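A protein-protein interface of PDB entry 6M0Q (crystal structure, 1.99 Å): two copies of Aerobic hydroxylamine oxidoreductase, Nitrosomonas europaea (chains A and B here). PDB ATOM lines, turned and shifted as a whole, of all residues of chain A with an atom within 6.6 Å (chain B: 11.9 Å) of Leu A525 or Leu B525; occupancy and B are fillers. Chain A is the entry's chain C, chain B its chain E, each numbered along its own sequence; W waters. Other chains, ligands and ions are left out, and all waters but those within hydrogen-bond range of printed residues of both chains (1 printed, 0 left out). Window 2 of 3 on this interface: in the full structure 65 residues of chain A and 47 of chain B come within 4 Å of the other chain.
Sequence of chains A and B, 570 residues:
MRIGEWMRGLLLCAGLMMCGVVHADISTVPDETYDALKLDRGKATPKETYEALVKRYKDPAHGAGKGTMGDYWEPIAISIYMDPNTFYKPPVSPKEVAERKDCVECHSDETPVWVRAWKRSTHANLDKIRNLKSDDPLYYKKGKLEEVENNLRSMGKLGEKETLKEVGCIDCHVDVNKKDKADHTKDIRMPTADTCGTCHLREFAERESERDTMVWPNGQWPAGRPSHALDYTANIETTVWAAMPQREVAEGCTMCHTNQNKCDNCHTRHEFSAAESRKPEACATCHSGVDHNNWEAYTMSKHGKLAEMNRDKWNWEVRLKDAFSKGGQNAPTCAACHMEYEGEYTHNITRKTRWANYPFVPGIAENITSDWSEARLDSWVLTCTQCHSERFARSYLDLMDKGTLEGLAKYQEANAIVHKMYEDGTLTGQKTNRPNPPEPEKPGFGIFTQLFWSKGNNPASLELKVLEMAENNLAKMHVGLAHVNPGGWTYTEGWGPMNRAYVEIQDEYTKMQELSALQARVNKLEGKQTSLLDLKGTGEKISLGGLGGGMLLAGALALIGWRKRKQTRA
The guanidinium group of Arg B521 lies within salt-bridge range of the side-chain carboxylate of Glu A526, at 3.2 Å.
Among the printed residues, merely in contact across the chains: Val A522 with Arg B521 (3.6 Å), Leu A525 with Leu B525 (3.8 Å), Val A522 with Val B522 (3.8 Å), Asn A523 with Arg B521 (3.8 Å), Val A522 with Leu B518 (3.9 Å), Glu A526 with Leu B525 (3.9 Å) and Val A522 with Leu B525 (3.996 Å).
Printed residues of chain B within 4 Å of Val A522: Leu B518 (3.9 Å), Arg B521 (3.6 Å), Val B522 (3.8 Å) and Leu B525 (3.996 Å). Of chain B, only Arg B521 comes within 4 Å of Asn A523. No residue of chain B comes within 4 Å of Lys A524. Leu A525 touches just one residue of chain B: Leu B525. No residue of chain B comes within 4 Å of Gly A527. No residue of chain B comes within 4 Å of Lys A528. Of the printed residues of chain A, Leu B518 touches Val A522. Gln B519 touches none of the printed residues of chain A. Gly B527 touches none of the printed residues of chain A. The nearest residue of chain B that does not touch Leu A525 is Val B522 (6.6 Å). The nearest printed residue of chain A that does not touch Leu B518 is Asn A523 (6.2 Å).
Of the 9 printed residues of chain A, 4 touch a printed residue of chain B. Printed residues of chain A that touch a printed residue of chain B: Val A522, Asn A523, Leu A525 and Glu A526. Of the 13 printed residues of chain B, 4 touch a printed residue of chain A. Hydrophobic or aromatic side chains of chain B within 4 Å of the printed part of chain A: Leu B518, Val B522 and Leu B525. Among the printed residues, 8 pairs touch across the chains. Among the printed residues, Asp or Glu carboxylates within 4 Å of a Lys or Arg side-chain nitrogen of the other chain: Glu A526 with Arg B521.
Val A522 touches Arg B521, but with the chains exchanged Arg A521 does not touch Val B522 (7.5 Å). Leu A525 touches its own counterpart, Leu B525. Glu A526 touches Arg B521, but with the chains exchanged Arg A521 does not touch Glu B526 (11.3 Å). Glu A526 touches Leu B525, but with the chains exchanged Leu A525 does not touch Glu B526 (8.0 Å). Of the 8 pairs that touch across the chains among the printed residues, 2 have their exchanged pair printed and touching as well.
Water W1 bridges the side-chain carboxylate of Glu A526 (2.5 Å) and the backbone carbonyl oxygen of Arg B521 (3.0 Å).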
ATOM      1  N   ALA A 520       1.046  -8.652  29.766  1.00  0.00           N
ATOM      2  CA  ALA A 520       0.510  -8.868  31.103  1.00  0.00           C
ATOM      3  C   ALA A 520      -0.995  -8.639  31.133  1.00  0.00           C
ATOM      4  O   ALA A 520      -1.728  -9.400  31.770  1.00  0.00           O
ATOM      5  CB  ALA A 520       1.219  -7.970  32.117  1.00  0.00           C
ATOM      6  N   ARG A 521      -1.486  -7.616  30.428  1.00  0.00           N
ATOM      7  CA  ARG A 521      -2.930  -7.404  30.394  1.00  0.00           C
ATOM      8  C   ARG A 521      -3.643  -8.568  29.706  1.00  0.00           C
ATOM      9  O   ARG A 521      -4.706  -9.013  30.157  1.00  0.00           O
ATOM     10  CB  ARG A 521      -3.250  -6.075  29.709  1.00  0.00           C
ATOM     11  CG  ARG A 521      -2.764  -4.868  30.495  1.00  0.00           C
ATOM     12  CD  ARG A 521      -2.818  -3.609  29.673  1.00  0.00           C
ATOM     13  NE  ARG A 521      -4.167  -3.269  29.232  1.00  0.00           N
ATOM     14  CZ  ARG A 521      -4.433  -2.468  28.200  1.00  0.00           C
ATOM     15  NH1 ARG A 521      -3.433  -1.934  27.503  1.00  0.00           N
ATOM     16  NH2 ARG A 521      -5.694  -2.203  27.855  1.00  0.00           N
ATOM     17  N   VAL A 522      -3.063  -9.095  28.629  1.00  0.00           N
ATOM     18  CA  VAL A 522      -3.694 -10.208  27.936  1.00  0.00           C
ATOM     19  C   VAL A 522      -3.592 -11.467  28.776  1.00  0.00           C
ATOM     20  O   VAL A 522      -4.525 -12.276  28.831  1.00  0.00           O
ATOM     21  CB  VAL A 522      -3.066 -10.374  26.546  1.00  0.00           C
ATOM     22  CG1 VAL A 522      -3.697 -11.543  25.778  1.00  0.00           C
ATOM     23  CG2 VAL A 522      -3.235  -9.081  25.785  1.00  0.00           C
ATOM     24  N   ASN A 523      -2.478 -11.633  29.480  1.00  0.00           N
ATOM     25  CA  ASN A 523      -2.363 -12.757  30.391  1.00  0.00           C
ATOM     26  C   ASN A 523      -3.397 -12.664  31.513  1.00  0.00           C
ATOM     27  O   ASN A 523      -4.008 -13.669  31.896  1.00  0.00           O
ATOM     28  CB  ASN A 523      -0.947 -12.815  30.946  1.00  0.00           C
ATOM     29  CG  ASN A 523      -0.631 -14.153  31.543  1.00  0.00           C
ATOM     30  OD1 ASN A 523      -0.265 -15.094  30.831  1.00  0.00           O
ATOM     31  ND2 ASN A 523      -0.798 -14.264  32.858  1.00  0.00           N
ATOM     32  N   LYS A 524      -3.627 -11.465  32.038  1.00  0.00           N
ATOM     33  CA  LYS A 524      -4.649 -11.313  33.063  1.00  0.00           C
ATOM     34  C   LYS A 524      -6.020 -11.688  32.522  1.00  0.00           C
ATOM     35  O   LYS A 524      -6.775 -12.406  33.183  1.00  0.00           O
ATOM     36  CB  LYS A 524      -4.648  -9.886  33.599  1.00  0.00           C
ATOM     37  CG  LYS A 524      -5.547  -9.676  34.797  1.00  0.00           C
ATOM     38  CD  LYS A 524      -5.425  -8.241  35.282  1.00  0.00           C
ATOM     39  CE  LYS A 524      -6.248  -7.969  36.525  1.00  0.00           C
ATOM     40  NZ  LYS A 524      -6.015  -6.569  36.986  1.00  0.00           N
ATOM     41  N   LEU A 525      -6.351 -11.235  31.308  1.00  0.00           N
ATOM     42  CA  LEU A 525      -7.642 -11.582  30.719  1.00  0.00           C
ATOM     43  C   LEU A 525      -7.781 -13.080  30.506  1.00  0.00           C
ATOM     44  O   LEU A 525      -8.897 -13.613  30.554  1.00  0.00           O
ATOM     45  CB  LEU A 525      -7.841 -10.862  29.388  1.00  0.00           C
ATOM     46  CG  LEU A 525      -7.960  -9.343  29.412  1.00  0.00           C
ATOM     47  CD1 LEU A 525      -8.124  -8.810  27.995  1.00  0.00           C
ATOM     48  CD2 LEU A 525      -9.115  -8.893  30.306  1.00  0.00           C
ATOM     49  N   GLU A 526      -6.675 -13.770  30.227  1.00  0.00           N
ATOM     50  CA  GLU A 526      -6.738 -15.215  30.078  1.00  0.00           C
ATOM     51  C   GLU A 526      -6.880 -15.911  31.421  1.00  0.00           C
ATOM     52  O   GLU A 526      -7.440 -17.009  31.481  1.00  0.00           O
ATOM     53  CB  GLU A 526      -5.504 -15.721  29.342  1.00  0.00           C
ATOM     54  CG  GLU A 526      -5.482 -15.356  27.872  1.00  0.00           C
ATOM     55  CD  GLU A 526      -4.138 -15.644  27.238  1.00  0.00           C
ATOM     56  OE1 GLU A 526      -3.155 -15.843  27.995  1.00  0.00           O
ATOM     57  OE2 GLU A 526      -4.066 -15.678  25.986  1.00  0.00           O
ATOM     58  N   GLY A 527      -6.399 -15.292  32.497  1.00  0.00           N
ATOM     59  CA  GLY A 527      -6.760 -15.740  33.823  1.00  0.00           C
ATOM     60  C   GLY A 527      -8.224 -15.577  34.158  1.00  0.00           C
ATOM     61  O   GLY A 527      -8.632 -15.963  35.256  1.00  0.00           O
ATOM     62  N   LYS A 528      -9.010 -14.989  33.251  1.00  0.00           N
ATOM     63  CA  LYS A 528     -10.473 -14.916  33.332  1.00  0.00           C
ATOM     64  C   LYS A 528     -10.951 -14.187  34.584  1.00  0.00           C
ATOM     65  O   LYS A 528     -10.737 -12.981  34.731  1.00  0.00           O
ATOM     66  CB  LYS A 528     -11.068 -16.330  33.256  1.00  0.00           C
ATOM     67  CG  LYS A 528     -10.701 -17.066  31.963  1.00  0.00           C
ATOM     68  CD  LYS A 528     -11.135 -18.524  31.971  1.00  0.00           C
ATOM     69  CE  LYS A 528     -10.733 -19.218  30.685  1.00  0.00           C
ATOM     70  NZ  LYS A 528     -11.257 -20.609  30.623  1.00  0.00           N
ATOM     71  N   SER B 516       2.640 -11.535  16.521  1.00  0.00           N
ATOM     72  CA  SER B 516       1.583 -12.332  15.911  1.00  0.00           C
ATOM     73  C   SER B 516       0.992 -13.314  16.907  1.00  0.00           C
ATOM     74  O   SER B 516      -0.220 -13.554  16.904  1.00  0.00           O
ATOM     75  CB  SER B 516       2.116 -13.075  14.690  1.00  0.00           C
ATOM     76  OG  SER B 516       2.238 -12.178  13.606  1.00  0.00           O
ATOM     77  N   ALA B 517       1.835 -13.893  17.762  1.00  0.00           N
ATOM     78  CA  ALA B 517       1.327 -14.774  18.807  1.00  0.00           C
ATOM     79  C   ALA B 517       0.423 -14.012  19.767  1.00  0.00           C
ATOM     80  O   ALA B 517      -0.644 -14.497  20.158  1.00  0.00           O
ATOM     81  CB  ALA B 517       2.491 -15.418  19.559  1.00  0.00           C
ATOM     82  N   LEU B 518       0.822 -12.810  20.150  1.00  0.00           N
ATOM     83  CA  LEU B 518      -0.023 -12.024  21.039  1.00  0.00           C
ATOM     84  C   LEU B 518      -1.336 -11.658  20.360  1.00  0.00           C
ATOM     85  O   LEU B 518      -2.408 -11.726  20.979  1.00  0.00           O
ATOM     86  CB  LEU B 518       0.724 -10.768  21.492  1.00  0.00           C
ATOM     87  CG  LEU B 518      -0.059  -9.923  22.487  1.00  0.00           C
ATOM     88  CD1 LEU B 518      -0.274 -10.704  23.777  1.00  0.00           C
ATOM     89  CD2 LEU B 518       0.684  -8.636  22.755  1.00  0.00           C
ATOM     90  N   GLN B 519      -1.273 -11.270  19.085  1.00  0.00           N
ATOM     91  CA  GLN B 519      -2.502 -10.980  18.372  1.00  0.00           C
ATOM     92  C   GLN B 519      -3.388 -12.218  18.286  1.00  0.00           C
ATOM     93  O   GLN B 519      -4.612 -12.117  18.417  1.00  0.00           O
ATOM     94  CB  GLN B 519      -2.183 -10.435  16.991  1.00  0.00           C
ATOM     95  CG  GLN B 519      -3.413  -9.972  16.245  1.00  0.00           C
ATOM     96  CD  GLN B 519      -3.106  -8.847  15.287  1.00  0.00           C
ATOM     97  OE1 GLN B 519      -2.008  -8.277  15.306  1.00  0.00           O
ATOM     98  NE2 GLN B 519      -4.079  -8.513  14.437  1.00  0.00           N
ATOM     99  N   ALA B 520      -2.786 -13.396  18.118  1.00  0.00           N
ATOM    100  CA  ALA B 520      -3.577 -14.622  18.066  1.00  0.00           C
ATOM    101  C   ALA B 520      -4.265 -14.891  19.395  1.00  0.00           C
ATOM    102  O   ALA B 520      -5.376 -15.434  19.416  1.00  0.00           O
ATOM    103  CB  ALA B 520      -2.701 -15.813  17.674  1.00  0.00           C
ATOM    104  N   ARG B 521      -3.633 -14.512  20.508  1.00  0.00           N
ATOM    105  CA  ARG B 521      -4.276 -14.717  21.801  1.00  0.00           C
ATOM    106  C   ARG B 521      -5.425 -13.735  21.995  1.00  0.00           C
ATOM    107  O   ARG B 521      -6.478 -14.098  22.536  1.00  0.00           O
ATOM    108  CB  ARG B 521      -3.245 -14.614  22.925  1.00  0.00           C
ATOM    109  CG  ARG B 521      -2.142 -15.657  22.805  1.00  0.00           C
ATOM    110  CD  ARG B 521      -1.283 -15.750  24.056  1.00  0.00           C
ATOM    111  NE  ARG B 521      -1.139 -14.476  24.733  1.00  0.00           N
ATOM    112  CZ  ARG B 521      -0.642 -14.333  25.955  1.00  0.00           C
ATOM    113  NH1 ARG B 521      -0.241 -15.386  26.640  1.00  0.00           N
ATOM    114  NH2 ARG B 521      -0.553 -13.135  26.505  1.00  0.00           N
ATOM    115  N   VAL B 522      -5.254 -12.495  21.538  1.00  0.00           N
ATOM    116  CA  VAL B 522      -6.341 -11.525  21.602  1.00  0.00           C
ATOM    117  C   VAL B 522      -7.474 -11.940  20.671  1.00  0.00           C
ATOM    118  O   VAL B 522      -8.644 -11.636  20.928  1.00  0.00           O
ATOM    119  CB  VAL B 522      -5.800 -10.120  21.277  1.00  0.00           C
ATOM    120  CG1 VAL B 522      -6.926  -9.103  21.219  1.00  0.00           C
ATOM    121  CG2 VAL B 522      -4.767  -9.707  22.334  1.00  0.00           C
ATOM    122  N   ASN B 523      -7.155 -12.648  19.586  1.00  0.00           N
ATOM    123  CA  ASN B 523      -8.201 -13.175  18.714  1.00  0.00           C
ATOM    124  C   ASN B 523      -8.985 -14.287  19.403  1.00  0.00           C
ATOM    125  O   ASN B 523     -10.213 -14.333  19.303  1.00  0.00           O
ATOM    126  CB  ASN B 523      -7.594 -13.665  17.398  1.00  0.00           C
ATOM    127  CG  ASN B 523      -7.822 -12.689  16.255  1.00  0.00           C
ATOM    128  OD1 ASN B 523      -7.002 -11.791  16.004  1.00  0.00           O
ATOM    129  ND2 ASN B 523      -8.942 -12.858  15.552  1.00  0.00           N
ATOM    130  N   LYS B 524      -8.298 -15.178  20.122  1.00  0.00           N
ATOM    131  CA  LYS B 524      -8.992 -16.188  20.915  1.00  0.00           C
ATOM    132  C   LYS B 524      -9.952 -15.550  21.908  1.00  0.00           C
ATOM    133  O   LYS B 524     -11.106 -15.975  22.033  1.00  0.00           O
ATOM    134  CB  LYS B 524      -7.988 -17.063  21.652  1.00  0.00           C
ATOM    135  CG  LYS B 524      -7.313 -18.084  20.775  1.00  0.00           C
ATOM    136  CD  LYS B 524      -6.644 -19.154  21.617  1.00  0.00           C
ATOM    137  CE  LYS B 524      -7.662 -19.961  22.414  1.00  0.00           C
ATOM    138  NZ  LYS B 524      -7.000 -21.091  23.135  1.00  0.00           N
ATOM    139  N   LEU B 525      -9.491 -14.524  22.631  1.00  0.00           N
ATOM    140  CA  LEU B 525     -10.358 -13.891  23.619  1.00  0.00           C
ATOM    141  C   LEU B 525     -11.567 -13.233  22.963  1.00  0.00           C
ATOM    142  O   LEU B 525     -12.669 -13.278  23.519  1.00  0.00           O
ATOM    143  CB  LEU B 525      -9.557 -12.890  24.456  1.00  0.00           C
ATOM    144  CG  LEU B 525      -8.455 -13.574  25.280  1.00  0.00           C
ATOM    145  CD1 LEU B 525      -7.550 -12.575  26.012  1.00  0.00           C
ATOM    146  CD2 LEU B 525      -9.042 -14.578  26.261  1.00  0.00           C
ATOM    147  N   GLU B 526     -11.401 -12.656  21.775  1.00  0.00           N
ATOM    148  CA  GLU B 526     -12.557 -12.143  21.052  1.00  0.00           C
ATOM    149  C   GLU B 526     -13.429 -13.241  20.459  1.00  0.00           C
ATOM    150  O   GLU B 526     -14.520 -12.937  19.968  1.00  0.00           O
ATOM    151  CB  GLU B 526     -12.113 -11.211  19.940  1.00  0.00           C
ATOM    152  CG  GLU B 526     -11.496  -9.942  20.419  1.00  0.00           C
ATOM    153  CD  GLU B 526     -10.814  -9.187  19.299  1.00  0.00           C
ATOM    154  OE1 GLU B 526     -10.562  -9.797  18.235  1.00  0.00           O
ATOM    155  OE2 GLU B 526     -10.528  -7.982  19.478  1.00  0.00           O
ATOM    156  N   GLY B 527     -12.973 -14.492  20.456  1.00  0.00           N
ATOM    157  CA  GLY B 527     -13.851 -15.568  20.047  1.00  0.00           C
ATOM    158  C   GLY B 527     -14.711 -16.132  21.157  1.00  0.00           C
ATOM    159  O   GLY B 527     -15.698 -16.818  20.871  1.00  0.00           O
ATOM    160  N   LYS B 528     -14.350 -15.858  22.414  1.00  0.00           N
ATOM    161  CA  LYS B 528     -15.101 -16.293  23.596  1.00  0.00           C
ATOM    162  C   LYS B 528     -16.043 -15.202  24.110  1.00  0.00           C
ATOM    163  O   LYS B 528     -17.219 -15.156  23.756  1.00  0.00           O
ATOM    164  CB  LYS B 528     -14.146 -16.694  24.723  1.00  0.00           C
ATOM    165  CG  LYS B 528     -13.117 -17.740  24.361  1.00  0.00           C
ATOM    166  CD  LYS B 528     -12.170 -17.975  25.534  1.00  0.00           C
ATOM    167  CE  LYS B 528     -11.175 -19.092  25.230  1.00  0.00           C
ATOM    168  NZ  LYS B 528     -10.292 -19.412  26.390  1.00  0.00           N
HETATM  169  O   HOH W   1      -5.880 -16.356  24.370  1.00  0.00           O
